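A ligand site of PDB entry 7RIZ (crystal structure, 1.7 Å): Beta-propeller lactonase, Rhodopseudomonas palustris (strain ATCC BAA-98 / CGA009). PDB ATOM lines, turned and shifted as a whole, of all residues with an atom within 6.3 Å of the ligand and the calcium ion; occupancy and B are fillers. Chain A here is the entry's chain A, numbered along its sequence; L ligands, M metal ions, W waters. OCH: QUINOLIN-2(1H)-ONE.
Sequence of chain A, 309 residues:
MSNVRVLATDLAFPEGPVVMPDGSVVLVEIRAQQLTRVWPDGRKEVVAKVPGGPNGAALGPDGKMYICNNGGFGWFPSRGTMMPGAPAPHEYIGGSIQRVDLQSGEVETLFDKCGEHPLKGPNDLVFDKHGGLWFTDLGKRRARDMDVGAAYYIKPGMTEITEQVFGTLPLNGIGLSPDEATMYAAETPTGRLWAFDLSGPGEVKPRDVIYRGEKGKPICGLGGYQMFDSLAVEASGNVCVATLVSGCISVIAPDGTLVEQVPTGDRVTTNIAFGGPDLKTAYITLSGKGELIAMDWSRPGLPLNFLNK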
ATOM      1  N   PHE A  13     -22.115  18.198   5.738  1.00  0.00           N
ATOM      2  CA  PHE A  13     -20.903  18.273   4.952  1.00  0.00           C
ATOM      3  C   PHE A  13     -21.282  18.641   3.518  1.00  0.00           C
ATOM      4  O   PHE A  13     -21.191  17.809   2.606  1.00  0.00           O
ATOM      5  CB  PHE A  13     -20.116  16.963   4.939  1.00  0.00           C
ATOM      6  CG  PHE A  13     -18.653  17.163   4.692  1.00  0.00           C
ATOM      7  CD1 PHE A  13     -18.146  17.254   3.415  1.00  0.00           C
ATOM      8  CD2 PHE A  13     -17.781  17.318   5.756  1.00  0.00           C
ATOM      9  CE1 PHE A  13     -16.807  17.461   3.171  1.00  0.00           C
ATOM     10  CE2 PHE A  13     -16.436  17.523   5.519  1.00  0.00           C
ATOM     11  CZ  PHE A  13     -15.938  17.586   4.256  1.00  0.00           C
ATOM     12  N   GLU A  15     -21.054  20.099  -0.269  1.00  0.00           N
ATOM     13  CA  GLU A  15     -20.049  20.075  -1.324  1.00  0.00           C
ATOM     14  C   GLU A  15     -20.818  20.226  -2.637  1.00  0.00           C
ATOM     15  O   GLU A  15     -22.047  20.323  -2.636  1.00  0.00           O
ATOM     16  CB  GLU A  15     -19.231  18.796  -1.300  1.00  0.00           C
ATOM     17  CG  GLU A  15     -17.754  18.984  -0.988  1.00  0.00           C
ATOM     18  CD  GLU A  15     -16.898  19.176  -2.232  1.00  0.00           C
ATOM     19  OE1 GLU A  15     -17.425  19.563  -3.295  1.00  0.00           O
ATOM     20  OE2 GLU A  15     -15.660  18.949  -2.155  1.00  0.00           O
ATOM     21  N   ILE A  30     -22.596  15.209   1.722  1.00  0.00           N
ATOM     22  CA  ILE A  30     -21.930  13.927   1.592  1.00  0.00           C
ATOM     23  C   ILE A  30     -22.369  13.011   2.720  1.00  0.00           C
ATOM     24  O   ILE A  30     -22.648  11.823   2.501  1.00  0.00           O
ATOM     25  CB  ILE A  30     -20.401  14.104   1.566  1.00  0.00           C
ATOM     26  CG1 ILE A  30     -19.994  15.226   0.650  1.00  0.00           C
ATOM     27  CG2 ILE A  30     -19.698  12.814   1.154  1.00  0.00           C
ATOM     28  CD1 ILE A  30     -18.472  15.313   0.454  1.00  0.00           C
ATOM     29  N   ASN A  55     -20.400  13.572  -3.912  1.00  0.00           N
ATOM     30  CA  ASN A  55     -19.227  14.420  -3.642  1.00  0.00           C
ATOM     31  C   ASN A  55     -19.161  15.637  -4.556  1.00  0.00           C
ATOM     32  O   ASN A  55     -18.663  16.691  -4.161  1.00  0.00           O
ATOM     33  CB  ASN A  55     -17.940  13.585  -3.828  1.00  0.00           C
ATOM     34  CG  ASN A  55     -16.735  14.091  -3.042  1.00  0.00           C
ATOM     35  OD1 ASN A  55     -15.890  13.270  -2.677  1.00  0.00           O
ATOM     36  ND2 ASN A  55     -16.631  15.385  -2.801  1.00  0.00           N
ATOM     37  N   ASN A  70     -18.332   9.076  -4.387  1.00  0.00           N
ATOM     38  CA  ASN A  70     -17.069   8.513  -3.964  1.00  0.00           C
ATOM     39  C   ASN A  70     -17.237   7.184  -3.252  1.00  0.00           C
ATOM     40  O   ASN A  70     -16.245   6.609  -2.810  1.00  0.00           O
ATOM     41  CB  ASN A  70     -16.325   9.527  -3.072  1.00  0.00           C
ATOM     42  CG  ASN A  70     -16.981   9.753  -1.721  1.00  0.00           C
ATOM     43  OD1 ASN A  70     -17.425   8.823  -1.017  1.00  0.00           O
ATOM     44  ND2 ASN A  70     -16.974  10.990  -1.313  1.00  0.00           N
ATOM     45  N   PHE A  73     -17.755   7.488   2.965  1.00  0.00           N
ATOM     46  CA  PHE A  73     -16.709   7.790   3.928  1.00  0.00           C
ATOM     47  C   PHE A  73     -17.105   7.203   5.278  1.00  0.00           C
ATOM     48  O   PHE A  73     -18.287   6.978   5.556  1.00  0.00           O
ATOM     49  CB  PHE A  73     -16.541   9.306   4.080  1.00  0.00           C
ATOM     50  CG  PHE A  73     -15.821   9.978   2.961  1.00  0.00           C
ATOM     51  CD1 PHE A  73     -14.683   9.435   2.418  1.00  0.00           C
ATOM     52  CD2 PHE A  73     -16.287  11.197   2.468  1.00  0.00           C
ATOM     53  CE1 PHE A  73     -14.004  10.087   1.424  1.00  0.00           C
ATOM     54  CE2 PHE A  73     -15.606  11.879   1.467  1.00  0.00           C
ATOM     55  CZ  PHE A  73     -14.482  11.310   0.902  1.00  0.00           C
ATOM     56  N   MET A  83     -15.878  14.696  10.552  1.00  0.00           N
ATOM     57  CA  MET A  83     -14.973  14.746   9.401  1.00  0.00           C
ATOM     58  C   MET A  83     -14.965  13.424   8.654  1.00  0.00           C
ATOM     59  O   MET A  83     -15.129  12.357   9.247  1.00  0.00           O
ATOM     60  CB  MET A  83     -13.543  15.104   9.819  1.00  0.00           C
ATOM     61  CG  MET A  83     -13.396  16.538  10.296  1.00  0.00           C
ATOM     62  SD  MET A  83     -13.622  17.747   8.969  1.00  0.00           S
ATOM     63  CE  MET A  83     -12.083  17.482   8.094  1.00  0.00           C
ATOM     64  N   PRO A  84     -14.791  13.462   7.344  1.00  0.00           N
ATOM     65  CA  PRO A  84     -14.679  12.213   6.594  1.00  0.00           C
ATOM     66  C   PRO A  84     -13.362  11.498   6.884  1.00  0.00           C
ATOM     67  O   PRO A  84     -12.312  12.113   7.071  1.00  0.00           O
ATOM     68  CB  PRO A  84     -14.787  12.664   5.120  1.00  0.00           C
ATOM     69  CG  PRO A  84     -14.364  14.104   5.118  1.00  0.00           C
ATOM     70  CD  PRO A  84     -14.805  14.640   6.464  1.00  0.00           C
ATOM     71  N   ASN A 123     -14.681  12.448  -7.301  1.00  0.00           N
ATOM     72  CA  ASN A 123     -14.744  13.628  -6.450  1.00  0.00           C
ATOM     73  C   ASN A 123     -15.467  14.812  -7.079  1.00  0.00           C
ATOM     74  O   ASN A 123     -16.447  15.275  -6.495  1.00  0.00           O
ATOM     75  CB  ASN A 123     -13.317  14.028  -5.990  1.00  0.00           C
ATOM     76  CG  ASN A 123     -13.342  15.067  -4.898  1.00  0.00           C
ATOM     77  OD1 ASN A 123     -13.775  16.188  -5.078  1.00  0.00           O
ATOM     78  ND2 ASN A 123     -12.874  14.697  -3.723  1.00  0.00           N
ATOM     79  N   ASP A 124     -14.949  15.389  -8.156  1.00  0.00           N
ATOM     80  CA  ASP A 124     -15.595  16.540  -8.783  1.00  0.00           C
ATOM     81  C   ASP A 124     -15.518  16.411 -10.302  1.00  0.00           C
ATOM     82  O   ASP A 124     -14.833  15.527 -10.855  1.00  0.00           O
ATOM     83  CB  ASP A 124     -14.959  17.833  -8.290  1.00  0.00           C
ATOM     84  CG  ASP A 124     -15.970  18.982  -8.165  1.00  0.00           C
ATOM     85  OD1 ASP A 124     -17.119  18.852  -8.671  1.00  0.00           O
ATOM     86  OD2 ASP A 124     -15.623  20.006  -7.506  1.00  0.00           O
ATOM     87  N   LEU A 138     -10.334  10.902  -6.309  1.00  0.00           N
ATOM     88  CA  LEU A 138      -9.469  11.141  -5.147  1.00  0.00           C
ATOM     89  C   LEU A 138      -8.836   9.871  -4.613  1.00  0.00           C
ATOM     90  O   LEU A 138      -7.847   9.942  -3.843  1.00  0.00           O
ATOM     91  CB  LEU A 138     -10.277  11.784  -4.033  1.00  0.00           C
ATOM     92  CG  LEU A 138      -9.548  12.400  -2.832  1.00  0.00           C
ATOM     93  CD1 LEU A 138      -8.890  13.699  -3.194  1.00  0.00           C
ATOM     94  CD2 LEU A 138     -10.513  12.589  -1.668  1.00  0.00           C
ATOM     95  N   ARG A 141      -9.041   5.940   1.084  1.00  0.00           N
ATOM     96  CA  ARG A 141      -8.083   5.608   2.148  1.00  0.00           C
ATOM     97  C   ARG A 141      -8.452   4.269   2.789  1.00  0.00           C
ATOM     98  O   ARG A 141      -9.627   3.960   2.968  1.00  0.00           O
ATOM     99  CB  ARG A 141      -8.089   6.705   3.213  1.00  0.00           C
ATOM    100  CG  ARG A 141      -7.426   8.013   2.794  1.00  0.00           C
ATOM    101  CD  ARG A 141      -7.952   9.158   3.665  1.00  0.00           C
ATOM    102  NE  ARG A 141      -9.401   9.337   3.474  1.00  0.00           N
ATOM    103  CZ  ARG A 141     -10.143  10.195   4.166  1.00  0.00           C
ATOM    104  NH1 ARG A 141      -9.596  10.987   5.086  1.00  0.00           N
ATOM    105  NH2 ARG A 141     -11.453  10.247   3.938  1.00  0.00           N
ATOM    106  N   ASN A 172      -8.727  16.274  -6.859  1.00  0.00           N
ATOM    107  CA  ASN A 172      -9.909  16.787  -6.190  1.00  0.00           C
ATOM    108  C   ASN A 172     -10.610  17.771  -7.116  1.00  0.00           C
ATOM    109  O   ASN A 172     -11.452  17.383  -7.932  1.00  0.00           O
ATOM    110  CB  ASN A 172      -9.495  17.405  -4.844  1.00  0.00           C
ATOM    111  CG  ASN A 172     -10.666  17.576  -3.900  1.00  0.00           C
ATOM    112  OD1 ASN A 172     -11.713  18.051  -4.280  1.00  0.00           O
ATOM    113  ND2 ASN A 172     -10.437  17.278  -2.612  1.00  0.00           N
ATOM    114  N   GLY A 173     -10.291  19.052  -7.016  1.00  0.00           N
ATOM    115  CA  GLY A 173     -10.917  20.022  -7.905  1.00  0.00           C
ATOM    116  C   GLY A 173     -10.529  19.828  -9.364  1.00  0.00           C
ATOM    117  O   GLY A 173      -9.423  19.418  -9.703  1.00  0.00           O
ATOM    118  N   ASP A 229      -8.904  21.518  -2.122  1.00  0.00           N
ATOM    119  CA  ASP A 229     -10.139  20.741  -2.301  1.00  0.00           C
ATOM    120  C   ASP A 229     -10.623  21.035  -3.717  1.00  0.00           C
ATOM    121  O   ASP A 229      -9.859  20.865  -4.668  1.00  0.00           O
ATOM    122  CB  ASP A 229     -11.138  21.097  -1.223  1.00  0.00           C
ATOM    123  CG  ASP A 229     -12.183  20.015  -1.028  1.00  0.00           C
ATOM    124  OD1 ASP A 229     -12.600  19.330  -1.993  1.00  0.00           O
ATOM    125  OD2 ASP A 229     -12.646  19.839   0.130  1.00  0.00           O
ATOM    126  N   SER A 230     -11.850  21.501  -3.885  1.00  0.00           N
ATOM    127  CA  SER A 230     -12.397  21.699  -5.219  1.00  0.00           C
ATOM    128  C   SER A 230     -12.190  23.128  -5.702  1.00  0.00           C
ATOM    129  O   SER A 230     -11.664  23.971  -4.981  1.00  0.00           O
ATOM    130  CB  SER A 230     -13.878  21.319  -5.199  1.00  0.00           C
ATOM    131  OG  SER A 230     -14.027  19.912  -5.351  1.00  0.00           O
ATOM    132  N   LEU A 244      -7.789  24.067   2.149  1.00  0.00           N
ATOM    133  CA  LEU A 244      -8.045  23.500   3.447  1.00  0.00           C
ATOM    134  C   LEU A 244      -6.917  23.892   4.378  1.00  0.00           C
ATOM    135  O   LEU A 244      -5.852  24.291   3.899  1.00  0.00           O
ATOM    136  CB  LEU A 244      -8.114  21.973   3.355  1.00  0.00           C
ATOM    137  CG  LEU A 244      -9.129  21.432   2.321  1.00  0.00           C
ATOM    138  CD1 LEU A 244      -8.736  20.029   1.919  1.00  0.00           C
ATOM    139  CD2 LEU A 244     -10.521  21.498   2.925  1.00  0.00           C
ATOM    140  N   VAL A 268     -12.084  23.905   6.884  1.00  0.00           N
ATOM    141  CA  VAL A 268     -12.566  22.916   5.930  1.00  0.00           C
ATOM    142  C   VAL A 268     -13.415  23.601   4.871  1.00  0.00           C
ATOM    143  O   VAL A 268     -14.603  23.290   4.730  1.00  0.00           O
ATOM    144  CB  VAL A 268     -13.383  21.809   6.628  1.00  0.00           C
ATOM    145  CG1 VAL A 268     -13.534  20.611   5.784  1.00  0.00           C
ATOM    146  CG2 VAL A 268     -12.690  21.418   7.980  1.00  0.00           C
ATOM    147  N   THR A 269     -12.816  24.525   4.137  1.00  0.00           N
ATOM    148  CA  THR A 269     -13.443  25.123   2.950  1.00  0.00           C
ATOM    149  C   THR A 269     -13.242  24.187   1.772  1.00  0.00           C
ATOM    150  O   THR A 269     -12.099  23.828   1.456  1.00  0.00           O
ATOM    151  CB  THR A 269     -12.791  26.485   2.694  1.00  0.00           C
ATOM    152  OG1 THR A 269     -13.019  27.304   3.835  1.00  0.00           O
ATOM    153  CG2 THR A 269     -13.389  27.147   1.445  1.00  0.00           C
ATOM    154  N   THR A 270     -14.364  23.811   1.061  1.00  0.00           N
ATOM    155  CA  THR A 270     -14.272  22.654   0.190  1.00  0.00           C
ATOM    156  C   THR A 270     -14.571  22.944  -1.270  1.00  0.00           C
ATOM    157  O   THR A 270     -14.011  22.270  -2.130  1.00  0.00           O
ATOM    158  CB  THR A 270     -15.212  21.535   0.664  1.00  0.00           C
ATOM    159  OG1 THR A 270     -16.574  21.997   0.725  1.00  0.00           O
ATOM    160  CG2 THR A 270     -14.788  21.019   2.056  1.00  0.00           C
ATOM    161  N   ASN A 271     -15.446  23.889  -1.572  1.00  0.00           N
ATOM    162  CA  ASN A 271     -15.758  24.141  -2.976  1.00  0.00           C
ATOM    163  C   ASN A 271     -16.233  25.578  -3.164  1.00  0.00           C
ATOM    164  O   ASN A 271     -16.585  26.291  -2.204  1.00  0.00           O
ATOM    165  CB  ASN A 271     -16.820  23.147  -3.482  1.00  0.00           C
ATOM    166  CG  ASN A 271     -16.675  22.809  -4.985  1.00  0.00           C
ATOM    167  OD1 ASN A 271     -16.275  23.628  -5.832  1.00  0.00           O
ATOM    168  ND2 ASN A 271     -16.972  21.576  -5.311  1.00  0.00           N
ATOM    169  N   SER A 287     -17.598  23.241   4.840  1.00  0.00           N
ATOM    170  CA  SER A 287     -18.088  21.912   5.194  1.00  0.00           C
ATOM    171  C   SER A 287     -17.846  21.607   6.659  1.00  0.00           C
ATOM    172  O   SER A 287     -18.552  20.771   7.212  1.00  0.00           O
ATOM    173  CB  SER A 287     -17.418  20.848   4.315  1.00  0.00           C
ATOM    174  OG  SER A 287     -17.784  21.074   2.924  1.00  0.00           O
HETATM  175  O1  OCH L   1     -14.058  16.503  -1.839  1.00  0.00           O
HETATM  176  N2  OCH L   1     -13.281  17.209   0.085  1.00  0.00           N
HETATM  177  C3  OCH L   1     -12.807  16.888   1.353  1.00  0.00           C
HETATM  178  C4  OCH L   1     -12.374  17.904   2.234  1.00  0.00           C
HETATM  179  C5  OCH L   1     -11.910  17.576   3.494  1.00  0.00           C
HETATM  180  C6  OCH L   1     -11.847  16.242   3.902  1.00  0.00           C
HETATM  181  C7  OCH L   1     -12.262  15.241   3.036  1.00  0.00           C
HETATM  182  C8  OCH L   1     -12.755  15.568   1.761  1.00  0.00           C
HETATM  183  C9  OCH L   1     -13.161  14.575   0.916  1.00  0.00           C
HETATM  184  C10 OCH L   1     -13.648  14.900  -0.338  1.00  0.00           C
HETATM  185  C1  OCH L   1     -13.701  16.241  -0.739  1.00  0.00           C
HETATM  186 CA    CA M   1     -14.027  18.152  -3.694  1.00  0.00          CA
HETATM  187  O   HOH W   1     -15.912  17.853  -5.032  1.00  0.00           O
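The side-chain carboxylate (OE1) of Glu 15 sits at hydrogen-bond distance from the side-chain amide nitrogen (ND2) of Asn 271. The side-chain amide oxygen (OD1) of Asn 55 lies within hydrogen-bond range of the side-chain amide nitrogen (ND2) of Asn 123. The backbone carbonyl oxygen of Thr 270 is in hydrogen-bond range of the backbone NH of Ser 230, 2.9 Å away. OG of Ser 230 lies close to OD2 of Asp 124. The side-chain hydroxyl (OG) of Ser 230 sits close to the side-chain amide nitrogen (ND2) of Asn 271 (3.4 Å). The backbone NH (N) of Gly 173 is in hydrogen-bond range of the backbone carbonyl oxygen (O) of Asp 229. The side-chain amide nitrogen (ND2) of Asn 70 sits at hydrogen-bond distance from the side-chain amide oxygen (OD1) of Asn 55. OG1 of Thr 270 lies within hydrogen-bond range of OG of Ser 287.
The calcium ion is bound by water W1 (2.3 Å), the side-chain carboxylate (OE2) of Glu 15 (2.4 Å), the side-chain amide oxygen (OD1) of Asn 172 (2.4 Å), the side-chain amide oxygen (OD1) of Asn 123 (2.4 Å), the side-chain hydroxyl (OG) of Ser 230 (2.4 Å), an oxygen (O1) of the ligand (2.5 Å) and the side-chain carboxylate (OD1) of Asp 229 (2.5 Å).
Merely in contact with the ligand: Pro 84 (3.2 Å), Phe 73 (3.5 Å) and Thr 270 (3.9 Å).
Asn 55 touches the calcium ion (ND2 to CA, 3.9 Å).
ND2 of Asn 55 lies close to O1 of the ligand (3.0 Å).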
